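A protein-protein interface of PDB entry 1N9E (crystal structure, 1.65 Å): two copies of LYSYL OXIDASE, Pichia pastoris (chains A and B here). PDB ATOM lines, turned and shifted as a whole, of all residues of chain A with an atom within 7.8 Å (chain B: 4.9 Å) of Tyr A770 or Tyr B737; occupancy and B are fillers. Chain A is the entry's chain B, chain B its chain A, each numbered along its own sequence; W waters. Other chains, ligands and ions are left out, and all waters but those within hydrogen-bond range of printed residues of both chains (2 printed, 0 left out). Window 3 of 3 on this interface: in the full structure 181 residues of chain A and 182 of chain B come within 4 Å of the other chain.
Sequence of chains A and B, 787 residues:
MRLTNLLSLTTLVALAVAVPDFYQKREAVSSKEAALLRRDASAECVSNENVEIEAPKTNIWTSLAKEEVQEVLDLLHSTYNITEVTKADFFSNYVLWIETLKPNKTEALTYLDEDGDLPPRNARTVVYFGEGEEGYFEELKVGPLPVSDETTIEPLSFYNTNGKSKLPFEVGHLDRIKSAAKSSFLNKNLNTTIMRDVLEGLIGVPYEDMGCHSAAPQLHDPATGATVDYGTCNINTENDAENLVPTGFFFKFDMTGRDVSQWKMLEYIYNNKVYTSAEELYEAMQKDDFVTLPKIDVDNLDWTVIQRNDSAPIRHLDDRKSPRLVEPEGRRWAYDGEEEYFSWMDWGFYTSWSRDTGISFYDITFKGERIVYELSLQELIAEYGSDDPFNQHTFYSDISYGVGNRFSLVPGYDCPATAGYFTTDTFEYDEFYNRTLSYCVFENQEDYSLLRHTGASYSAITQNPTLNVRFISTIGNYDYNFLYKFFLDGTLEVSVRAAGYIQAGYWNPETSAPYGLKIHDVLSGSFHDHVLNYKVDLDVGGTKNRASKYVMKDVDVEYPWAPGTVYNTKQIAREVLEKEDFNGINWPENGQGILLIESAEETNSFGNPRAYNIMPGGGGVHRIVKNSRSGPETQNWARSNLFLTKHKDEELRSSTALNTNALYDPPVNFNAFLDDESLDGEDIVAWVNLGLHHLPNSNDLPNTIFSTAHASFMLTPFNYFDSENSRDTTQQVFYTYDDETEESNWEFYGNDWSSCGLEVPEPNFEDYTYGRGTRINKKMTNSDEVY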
ATOM      1  N   ASP A 240      19.070 -31.900 -29.930  1.00  0.00           N
ATOM      2  CA  ASP A 240      19.015 -32.944 -28.886  1.00  0.00           C
ATOM      3  C   ASP A 240      19.652 -34.236 -29.397  1.00  0.00           C
ATOM      4  O   ASP A 240      19.289 -35.336 -28.965  1.00  0.00           O
ATOM      5  CB  ASP A 240      17.558 -33.200 -28.427  1.00  0.00           C
ATOM      6  CG  ASP A 240      17.464 -34.071 -27.175  1.00  0.00           C
ATOM      7  OD1 ASP A 240      18.150 -33.760 -26.176  1.00  0.00           O
ATOM      8  OD2 ASP A 240      16.732 -35.093 -27.096  1.00  0.00           O
ATOM      9  N   PHE A 407       6.372 -36.007 -20.838  1.00  0.00           N
ATOM     10  CA  PHE A 407       5.636 -35.044 -21.660  1.00  0.00           C
ATOM     11  C   PHE A 407       4.252 -35.471 -22.108  1.00  0.00           C
ATOM     12  O   PHE A 407       3.859 -36.626 -21.979  1.00  0.00           O
ATOM     13  CB  PHE A 407       6.384 -34.769 -22.963  1.00  0.00           C
ATOM     14  CG  PHE A 407       7.830 -34.329 -22.826  1.00  0.00           C
ATOM     15  CD1 PHE A 407       8.847 -35.263 -22.664  1.00  0.00           C
ATOM     16  CD2 PHE A 407       8.169 -32.982 -22.874  1.00  0.00           C
ATOM     17  CE1 PHE A 407      10.168 -34.867 -22.546  1.00  0.00           C
ATOM     18  CE2 PHE A 407       9.500 -32.572 -22.756  1.00  0.00           C
ATOM     19  CZ  PHE A 407      10.499 -33.514 -22.593  1.00  0.00           C
ATOM     20  N   SER A 408       3.506 -34.511 -22.652  1.00  0.00           N
ATOM     21  CA  SER A 408       2.182 -34.793 -23.189  1.00  0.00           C
ATOM     22  C   SER A 408       2.245 -35.552 -24.498  1.00  0.00           C
ATOM     23  O   SER A 408       3.264 -35.545 -25.184  1.00  0.00           O
ATOM     24  CB  SER A 408       1.485 -33.471 -23.539  1.00  0.00           C
ATOM     25  OG  SER A 408       1.182 -32.715 -22.388  1.00  0.00           O
ATOM     26  N   THR A 474       9.090 -40.151 -22.917  1.00  0.00           N
ATOM     27  CA  THR A 474      10.352 -39.782 -23.533  1.00  0.00           C
ATOM     28  C   THR A 474      11.315 -39.421 -22.400  1.00  0.00           C
ATOM     29  O   THR A 474      11.118 -38.416 -21.723  1.00  0.00           O
ATOM     30  CB  THR A 474      10.184 -38.554 -24.441  1.00  0.00           C
ATOM     31  OG1 THR A 474       9.223 -38.834 -25.477  1.00  0.00           O
ATOM     32  CG2 THR A 474      11.491 -38.296 -25.191  1.00  0.00           C
ATOM     33  N   ASP A 767      -4.363 -28.211 -27.400  1.00  0.00           N
ATOM     34  CA  ASP A 767      -4.135 -28.689 -26.034  1.00  0.00           C
ATOM     35  C   ASP A 767      -2.688 -29.123 -25.797  1.00  0.00           C
ATOM     36  O   ASP A 767      -2.280 -29.342 -24.651  1.00  0.00           O
ATOM     37  CB  ASP A 767      -5.021 -29.908 -25.721  1.00  0.00           C
ATOM     38  CG  ASP A 767      -6.481 -29.561 -25.567  1.00  0.00           C
ATOM     39  OD1 ASP A 767      -6.791 -28.362 -25.429  1.00  0.00           O
ATOM     40  OD2 ASP A 767      -7.385 -30.432 -25.571  1.00  0.00           O
ATOM     41  N   TYR A 768      -1.921 -29.254 -26.869  1.00  0.00           N
ATOM     42  CA  TYR A 768      -0.535 -29.695 -26.746  1.00  0.00           C
ATOM     43  C   TYR A 768       0.429 -28.540 -26.628  1.00  0.00           C
ATOM     44  O   TYR A 768       0.567 -27.740 -27.541  1.00  0.00           O
ATOM     45  CB  TYR A 768      -0.118 -30.532 -27.945  1.00  0.00           C
ATOM     46  CG  TYR A 768       1.307 -31.053 -27.827  1.00  0.00           C
ATOM     47  CD1 TYR A 768       1.599 -32.170 -27.041  1.00  0.00           C
ATOM     48  CD2 TYR A 768       2.357 -30.433 -28.499  1.00  0.00           C
ATOM     49  CE1 TYR A 768       2.890 -32.650 -26.927  1.00  0.00           C
ATOM     50  CE2 TYR A 768       3.652 -30.903 -28.394  1.00  0.00           C
ATOM     51  CZ  TYR A 768       3.914 -32.014 -27.606  1.00  0.00           C
ATOM     52  OH  TYR A 768       5.204 -32.484 -27.501  1.00  0.00           O
ATOM     53  N   THR A 769       1.097 -28.466 -25.491  1.00  0.00           N
ATOM     54  CA  THR A 769       2.192 -27.535 -25.339  1.00  0.00           C
ATOM     55  C   THR A 769       3.422 -28.288 -24.845  1.00  0.00           C
ATOM     56  O   THR A 769       3.312 -29.207 -24.032  1.00  0.00           O
ATOM     57  CB  THR A 769       1.835 -26.477 -24.309  1.00  0.00           C
ATOM     58  OG1 THR A 769       0.673 -25.757 -24.749  1.00  0.00           O
ATOM     59  CG2 THR A 769       2.938 -25.413 -24.256  1.00  0.00           C
ATOM     60  N   TYR A 770       4.589 -27.897 -25.331  1.00  0.00           N
ATOM     61  CA  TYR A 770       5.825 -28.546 -24.936  1.00  0.00           C
ATOM     62  C   TYR A 770       6.069 -28.467 -23.434  1.00  0.00           C
ATOM     63  O   TYR A 770       5.674 -27.506 -22.774  1.00  0.00           O
ATOM     64  CB  TYR A 770       7.006 -27.905 -25.655  1.00  0.00           C
ATOM     65  CG  TYR A 770       8.302 -28.659 -25.472  1.00  0.00           C
ATOM     66  CD1 TYR A 770       8.584 -29.789 -26.238  1.00  0.00           C
ATOM     67  CD2 TYR A 770       9.250 -28.246 -24.532  1.00  0.00           C
ATOM     68  CE1 TYR A 770       9.765 -30.479 -26.074  1.00  0.00           C
ATOM     69  CE2 TYR A 770      10.438 -28.937 -24.362  1.00  0.00           C
ATOM     70  CZ  TYR A 770      10.686 -30.056 -25.140  1.00  0.00           C
ATOM     71  OH  TYR A 770      11.855 -30.755 -24.991  1.00  0.00           O
ATOM     72  N   GLY A 771       6.723 -29.486 -22.893  1.00  0.00           N
ATOM     73  CA  GLY A 771       7.128 -29.420 -21.502  1.00  0.00           C
ATOM     74  C   GLY A 771       6.745 -30.596 -20.642  1.00  0.00           C
ATOM     75  O   GLY A 771       5.868 -31.395 -20.985  1.00  0.00           O
ATOM     76  N   ARG A 772       7.413 -30.707 -19.501  1.00  0.00           N
ATOM     77  CA  ARG A 772       7.158 -31.831 -18.615  1.00  0.00           C
ATOM     78  C   ARG A 772       6.147 -31.561 -17.496  1.00  0.00           C
ATOM     79  O   ARG A 772       6.420 -31.835 -16.326  1.00  0.00           O
ATOM     80  CB  ARG A 772       8.471 -32.385 -18.068  1.00  0.00           C
ATOM     81  CG  ARG A 772       9.414 -32.889 -19.163  1.00  0.00           C
ATOM     82  CD  ARG A 772      10.776 -33.296 -18.618  1.00  0.00           C
ATOM     83  NE  ARG A 772      10.611 -34.104 -17.412  1.00  0.00           N
ATOM     84  CZ  ARG A 772      11.569 -34.364 -16.530  1.00  0.00           C
ATOM     85  NH1 ARG A 772      12.796 -33.880 -16.699  1.00  0.00           N
ATOM     86  NH2 ARG A 772      11.292 -35.112 -15.469  1.00  0.00           N
ATOM     87  N   GLY A 773       4.986 -31.027 -17.868  1.00  0.00           N
ATOM     88  CA  GLY A 773       3.942 -30.687 -16.911  1.00  0.00           C
ATOM     89  C   GLY A 773       3.882 -29.211 -16.531  1.00  0.00           C
ATOM     90  O   GLY A 773       4.856 -28.476 -16.690  1.00  0.00           O
ATOM     91  N   THR A 774       2.730 -28.777 -16.028  1.00  0.00           N
ATOM     92  CA  THR A 774       2.547 -27.400 -15.568  1.00  0.00           C
ATOM     93  C   THR A 774       2.757 -27.391 -14.061  1.00  0.00           C
ATOM     94  O   THR A 774       2.063 -28.098 -13.330  1.00  0.00           O
ATOM     95  CB  THR A 774       1.138 -26.893 -15.923  1.00  0.00           C
ATOM     96  OG1 THR A 774       1.071 -26.635 -17.331  1.00  0.00           O
ATOM     97  CG2 THR A 774       0.892 -25.523 -15.306  1.00  0.00           C
ATOM     98  N   THR B 454      10.847 -36.349 -28.854  1.00  0.00           N
ATOM     99  CA  THR B 454      10.553 -35.040 -28.276  1.00  0.00           C
ATOM    100  C   THR B 454      11.838 -34.641 -27.612  1.00  0.00           C
ATOM    101  O   THR B 454      12.358 -35.356 -26.763  1.00  0.00           O
ATOM    102  CB  THR B 454       9.453 -35.152 -27.213  1.00  0.00           C
ATOM    103  OG1 THR B 454       8.195 -35.372 -27.860  1.00  0.00           O
ATOM    104  CG2 THR B 454       9.271 -33.814 -26.460  1.00  0.00           C
ATOM    105  N   GLY B 455      12.373 -33.497 -27.995  1.00  0.00           N
ATOM    106  CA  GLY B 455      13.436 -32.960 -27.180  1.00  0.00           C
ATOM    107  C   GLY B 455      13.795 -31.581 -27.620  1.00  0.00           C
ATOM    108  O   GLY B 455      13.370 -31.153 -28.683  1.00  0.00           O
ATOM    109  N   ALA B 456      14.573 -30.883 -26.801  1.00  0.00           N
ATOM    110  CA  ALA B 456      15.141 -29.641 -27.260  1.00  0.00           C
ATOM    111  C   ALA B 456      14.098 -28.739 -27.933  1.00  0.00           C
ATOM    112  O   ALA B 456      14.354 -28.166 -28.996  1.00  0.00           O
ATOM    113  CB  ALA B 456      16.309 -29.951 -28.219  1.00  0.00           C
ATOM    114  N   SER B 457      12.931 -28.629 -27.302  1.00  0.00           N
ATOM    115  CA  SER B 457      11.874 -27.725 -27.759  1.00  0.00           C
ATOM    116  C   SER B 457      11.194 -28.100 -29.069  1.00  0.00           C
ATOM    117  O   SER B 457      10.613 -27.242 -29.760  1.00  0.00           O
ATOM    118  CB  SER B 457      12.399 -26.287 -27.826  1.00  0.00           C
ATOM    119  OG  SER B 457      12.806 -25.885 -26.535  1.00  0.00           O
ATOM    120  N   TYR B 458      11.260 -29.379 -29.427  1.00  0.00           N
ATOM    121  CA  TYR B 458      10.503 -29.817 -30.579  1.00  0.00           C
ATOM    122  C   TYR B 458       9.926 -31.205 -30.338  1.00  0.00           C
ATOM    123  O   TYR B 458      10.363 -31.927 -29.439  1.00  0.00           O
ATOM    124  CB  TYR B 458      11.373 -29.840 -31.860  1.00  0.00           C
ATOM    125  CG  TYR B 458      12.426 -30.936 -31.843  1.00  0.00           C
ATOM    126  CD1 TYR B 458      12.116 -32.237 -32.242  1.00  0.00           C
ATOM    127  CD2 TYR B 458      13.731 -30.665 -31.423  1.00  0.00           C
ATOM    128  CE1 TYR B 458      13.081 -33.236 -32.223  1.00  0.00           C
ATOM    129  CE2 TYR B 458      14.708 -31.661 -31.403  1.00  0.00           C
ATOM    130  CZ  TYR B 458      14.375 -32.938 -31.803  1.00  0.00           C
ATOM    131  OH  TYR B 458      15.330 -33.920 -31.781  1.00  0.00           O
ATOM    132  N   SER B 459       8.936 -31.549 -31.157  1.00  0.00           N
ATOM    133  CA  SER B 459       8.441 -32.926 -31.250  1.00  0.00           C
ATOM    134  C   SER B 459       8.331 -33.284 -32.729  1.00  0.00           C
ATOM    135  O   SER B 459       7.712 -32.556 -33.517  1.00  0.00           O
ATOM    136  CB  SER B 459       7.110 -33.107 -30.527  1.00  0.00           C
ATOM    137  OG  SER B 459       7.295 -33.016 -29.133  1.00  0.00           O
ATOM    138  N   TYR B 735       6.736 -30.158 -34.769  1.00  0.00           N
ATOM    139  CA  TYR B 735       6.233 -29.168 -33.825  1.00  0.00           C
ATOM    140  C   TYR B 735       7.436 -28.493 -33.157  1.00  0.00           C
ATOM    141  O   TYR B 735       8.370 -29.168 -32.718  1.00  0.00           O
ATOM    142  CB  TYR B 735       5.355 -29.860 -32.754  1.00  0.00           C
ATOM    143  CG  TYR B 735       5.085 -28.978 -31.546  1.00  0.00           C
ATOM    144  CD1 TYR B 735       6.011 -28.885 -30.512  1.00  0.00           C
ATOM    145  CD2 TYR B 735       3.913 -28.236 -31.442  1.00  0.00           C
ATOM    146  CE1 TYR B 735       5.782 -28.078 -29.395  1.00  0.00           C
ATOM    147  CE2 TYR B 735       3.674 -27.423 -30.328  1.00  0.00           C
ATOM    148  CZ  TYR B 735       4.614 -27.352 -29.312  1.00  0.00           C
ATOM    149  OH  TYR B 735       4.397 -26.553 -28.199  1.00  0.00           O
ATOM    150  N   THR B 736       7.432 -27.163 -33.074  1.00  0.00           N
ATOM    151  CA  THR B 736       8.493 -26.474 -32.360  1.00  0.00           C
ATOM    152  C   THR B 736       7.874 -25.465 -31.392  1.00  0.00           C
ATOM    153  O   THR B 736       6.775 -24.947 -31.634  1.00  0.00           O
ATOM    154  CB  THR B 736       9.445 -25.732 -33.333  1.00  0.00           C
ATOM    155  OG1 THR B 736       8.677 -24.972 -34.278  1.00  0.00           O
ATOM    156  CG2 THR B 736      10.186 -26.698 -34.223  1.00  0.00           C
ATOM    157  N   TYR B 737       8.582 -25.195 -30.304  1.00  0.00           N
ATOM    158  CA  TYR B 737       8.129 -24.239 -29.303  1.00  0.00           C
ATOM    159  C   TYR B 737       9.202 -23.189 -29.108  1.00  0.00           C
ATOM    160  O   TYR B 737      10.376 -23.524 -28.931  1.00  0.00           O
ATOM    161  CB  TYR B 737       7.840 -24.912 -27.970  1.00  0.00           C
ATOM    162  CG  TYR B 737       7.330 -23.943 -26.935  1.00  0.00           C
ATOM    163  CD1 TYR B 737       6.025 -23.471 -26.990  1.00  0.00           C
ATOM    164  CD2 TYR B 737       8.148 -23.497 -25.907  1.00  0.00           C
ATOM    165  CE1 TYR B 737       5.547 -22.586 -26.053  1.00  0.00           C
ATOM    166  CE2 TYR B 737       7.678 -22.607 -24.959  1.00  0.00           C
ATOM    167  CZ  TYR B 737       6.374 -22.157 -25.040  1.00  0.00           C
ATOM    168  OH  TYR B 737       5.885 -21.272 -24.109  1.00  0.00           O
ATOM    169  N   ASP B 738       8.792 -21.922 -29.139  1.00  0.00           N
ATOM    170  CA  ASP B 738       9.732 -20.816 -29.034  1.00  0.00           C
ATOM    171  C   ASP B 738       9.823 -20.308 -27.617  1.00  0.00           C
ATOM    172  O   ASP B 738       8.914 -19.657 -27.108  1.00  0.00           O
ATOM    173  CB  ASP B 738       9.363 -19.656 -29.956  1.00  0.00           C
ATOM    174  CG  ASP B 738      10.375 -18.524 -29.881  1.00  0.00           C
ATOM    175  OD1 ASP B 738      10.628 -17.878 -30.918  1.00  0.00           O
ATOM    176  OD2 ASP B 738      10.968 -18.213 -28.825  1.00  0.00           O
ATOM    177  N   ASP B 739      10.948 -20.620 -27.000  1.00  0.00           N
ATOM    178  CA  ASP B 739      11.220 -20.323 -25.609  1.00  0.00           C
ATOM    179  C   ASP B 739      11.106 -18.860 -25.194  1.00  0.00           C
ATOM    180  O   ASP B 739      10.775 -18.563 -24.044  1.00  0.00           O
ATOM    181  CB  ASP B 739      12.669 -20.745 -25.311  1.00  0.00           C
ATOM    182  CG  ASP B 739      12.998 -22.142 -25.817  1.00  0.00           C
ATOM    183  OD1 ASP B 739      12.249 -22.673 -26.668  1.00  0.00           O
ATOM    184  OD2 ASP B 739      13.993 -22.788 -25.417  1.00  0.00           O
ATOM    185  N   GLU B 742       7.121 -17.986 -26.278  1.00  0.00           N
ATOM    186  CA  GLU B 742       6.146 -18.942 -25.767  1.00  0.00           C
ATOM    187  C   GLU B 742       5.134 -19.258 -26.884  1.00  0.00           C
ATOM    188  O   GLU B 742       3.963 -19.535 -26.622  1.00  0.00           O
ATOM    189  CB  GLU B 742       5.449 -18.414 -24.504  1.00  0.00           C
ATOM    190  CG  GLU B 742       6.408 -18.136 -23.350  1.00  0.00           C
ATOM    191  CD  GLU B 742       5.751 -18.214 -21.979  1.00  0.00           C
ATOM    192  OE1 GLU B 742       5.246 -19.297 -21.613  1.00  0.00           O
ATOM    193  OE2 GLU B 742       5.741 -17.188 -21.262  1.00  0.00           O
ATOM    194  N   GLU B 743       5.612 -19.208 -28.129  1.00  0.00           N
ATOM    195  CA  GLU B 743       4.792 -19.471 -29.316  1.00  0.00           C
ATOM    196  C   GLU B 743       5.099 -20.853 -29.904  1.00  0.00           C
ATOM    197  O   GLU B 743       6.259 -21.197 -30.084  1.00  0.00           O
ATOM    198  CB  GLU B 743       5.057 -18.402 -30.365  1.00  0.00           C
ATOM    199  CG  GLU B 743       3.932 -18.211 -31.362  1.00  0.00           C
ATOM    200  CD  GLU B 743       4.048 -16.891 -32.094  1.00  0.00           C
ATOM    201  OE1 GLU B 743       3.749 -15.844 -31.478  1.00  0.00           O
ATOM    202  OE2 GLU B 743       4.439 -16.903 -33.282  1.00  0.00           O
ATOM    203  N   SER B 744       4.055 -21.630 -30.193  1.00  0.00           N
ATOM    204  CA  SER B 744       4.189 -22.934 -30.863  1.00  0.00           C
ATOM    205  C   SER B 744       4.076 -22.787 -32.391  1.00  0.00           C
ATOM    206  O   SER B 744       3.387 -21.889 -32.881  1.00  0.00           O
ATOM    207  CB  SER B 744       3.115 -23.899 -30.362  1.00  0.00           C
ATOM    208  OG  SER B 744       3.342 -24.251 -29.005  1.00  0.00           O
HETATM  209  O   HOH W   1       5.500 -35.008 -26.657  1.00  0.00           O
HETATM  210  O   HOH W   2       6.889 -37.389 -25.341  1.00  0.00           O
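OH of Tyr A768 sits at hydrogen-bond distance from OG of Ser B459.
The side-chain hydroxyl (OH) of Tyr A770 sits at hydrogen-bond distance from the backbone NH (N) of Ser B457, 3.3 Å away.
The side-chain hydroxyl of Tyr A770 is in hydrogen-bond range of the backbone NH of Ala B456 (3.3 Å).
The side-chain hydroxyl of Tyr B735 is in hydrogen-bond range of the backbone NH of Tyr A770 (3.2 Å).
OD1 of Asp B739 is in hydrogen-bond range of OG of Ser B457, at 3.3 Å.
The backbone carbonyl oxygen (O) of Ser B459 sits at hydrogen-bond distance from the backbone NH (N) of Tyr B735, at 2.9 Å.
OG1 of Thr B454 lies within hydrogen-bond range of OG of Ser B459, 2.8 Å away.
OH of Tyr B737 sits close to OE1 of Glu B742 (3.2 Å).
The side-chain hydroxyl of Tyr B735 sits at hydrogen-bond distance from the side-chain hydroxyl of Ser B744 (2.7 Å).
The backbone NH (N) of Tyr B737 lies within hydrogen-bond range of the backbone carbonyl oxygen (O) of Ser B457, at 2.9 Å.
Asp A240 touches Gly B455.
Asp A240 touches Ala B456 (CB to CB, 3.5 Å).
Phe A407 touches Thr B454 (CD2 to CG2, 3.8 Å).
Thr A474 touches Thr B454 (CG2 to O, 3.4 Å).
Tyr B735 touches Tyr A768.
OH of Tyr B735 touches CA of Thr A769, 3.7 Å away.
Tyr A770 touches Thr B454.
OH of Tyr A770 touches C of Gly B455 (3.4 Å).
Tyr B458 touches Tyr A770 (O to CE1, 3.7 Å).
Tyr A770 touches Tyr B737 (CB to CB, 3.9 Å).
Of the printed residues of chain A, Thr B454 touches Phe A407 (3.8 Å), Thr A474 (3.4 Å) and Tyr A770 (3.4 Å).
Of the printed residues of chain A, Gly B455 touches Asp A240 (3.9 Å) and Tyr A770 (3.4 Å).
Of chain A, only Tyr A770 comes within 4 Å of Tyr B737.
Asp B738 touches none of the printed residues of chain A.
The nearest printed residue of chain B that does not touch Thr A769 is Tyr B737 (4.2 Å).
Of the 14 printed residues of chain B, 8 touch a printed residue of chain A.
Hydrophobic or aromatic side chains of chain B within 4 Å of the printed part of chain A: Ala B456, Tyr B735 and Tyr B737.
Of the 12 printed residues of chain A, 6 touch a printed residue of chain B.
Among the printed residues, 14 pairs touch across the chains.
Among the printed residues, no Asp or Glu carboxylate lies within 4 Å of a Lys or Arg side-chain nitrogen of the other chain.
No position is printed for both chains.
Water W1 lies within hydrogen-bond range of OH of Tyr A768, O of Ser A408 and OG1 of Thr B454.
Water W2 lies within hydrogen-bond range of OG1 of Thr A474 (2.7 Å) and OG1 of Thr B454 (3.5 Å).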
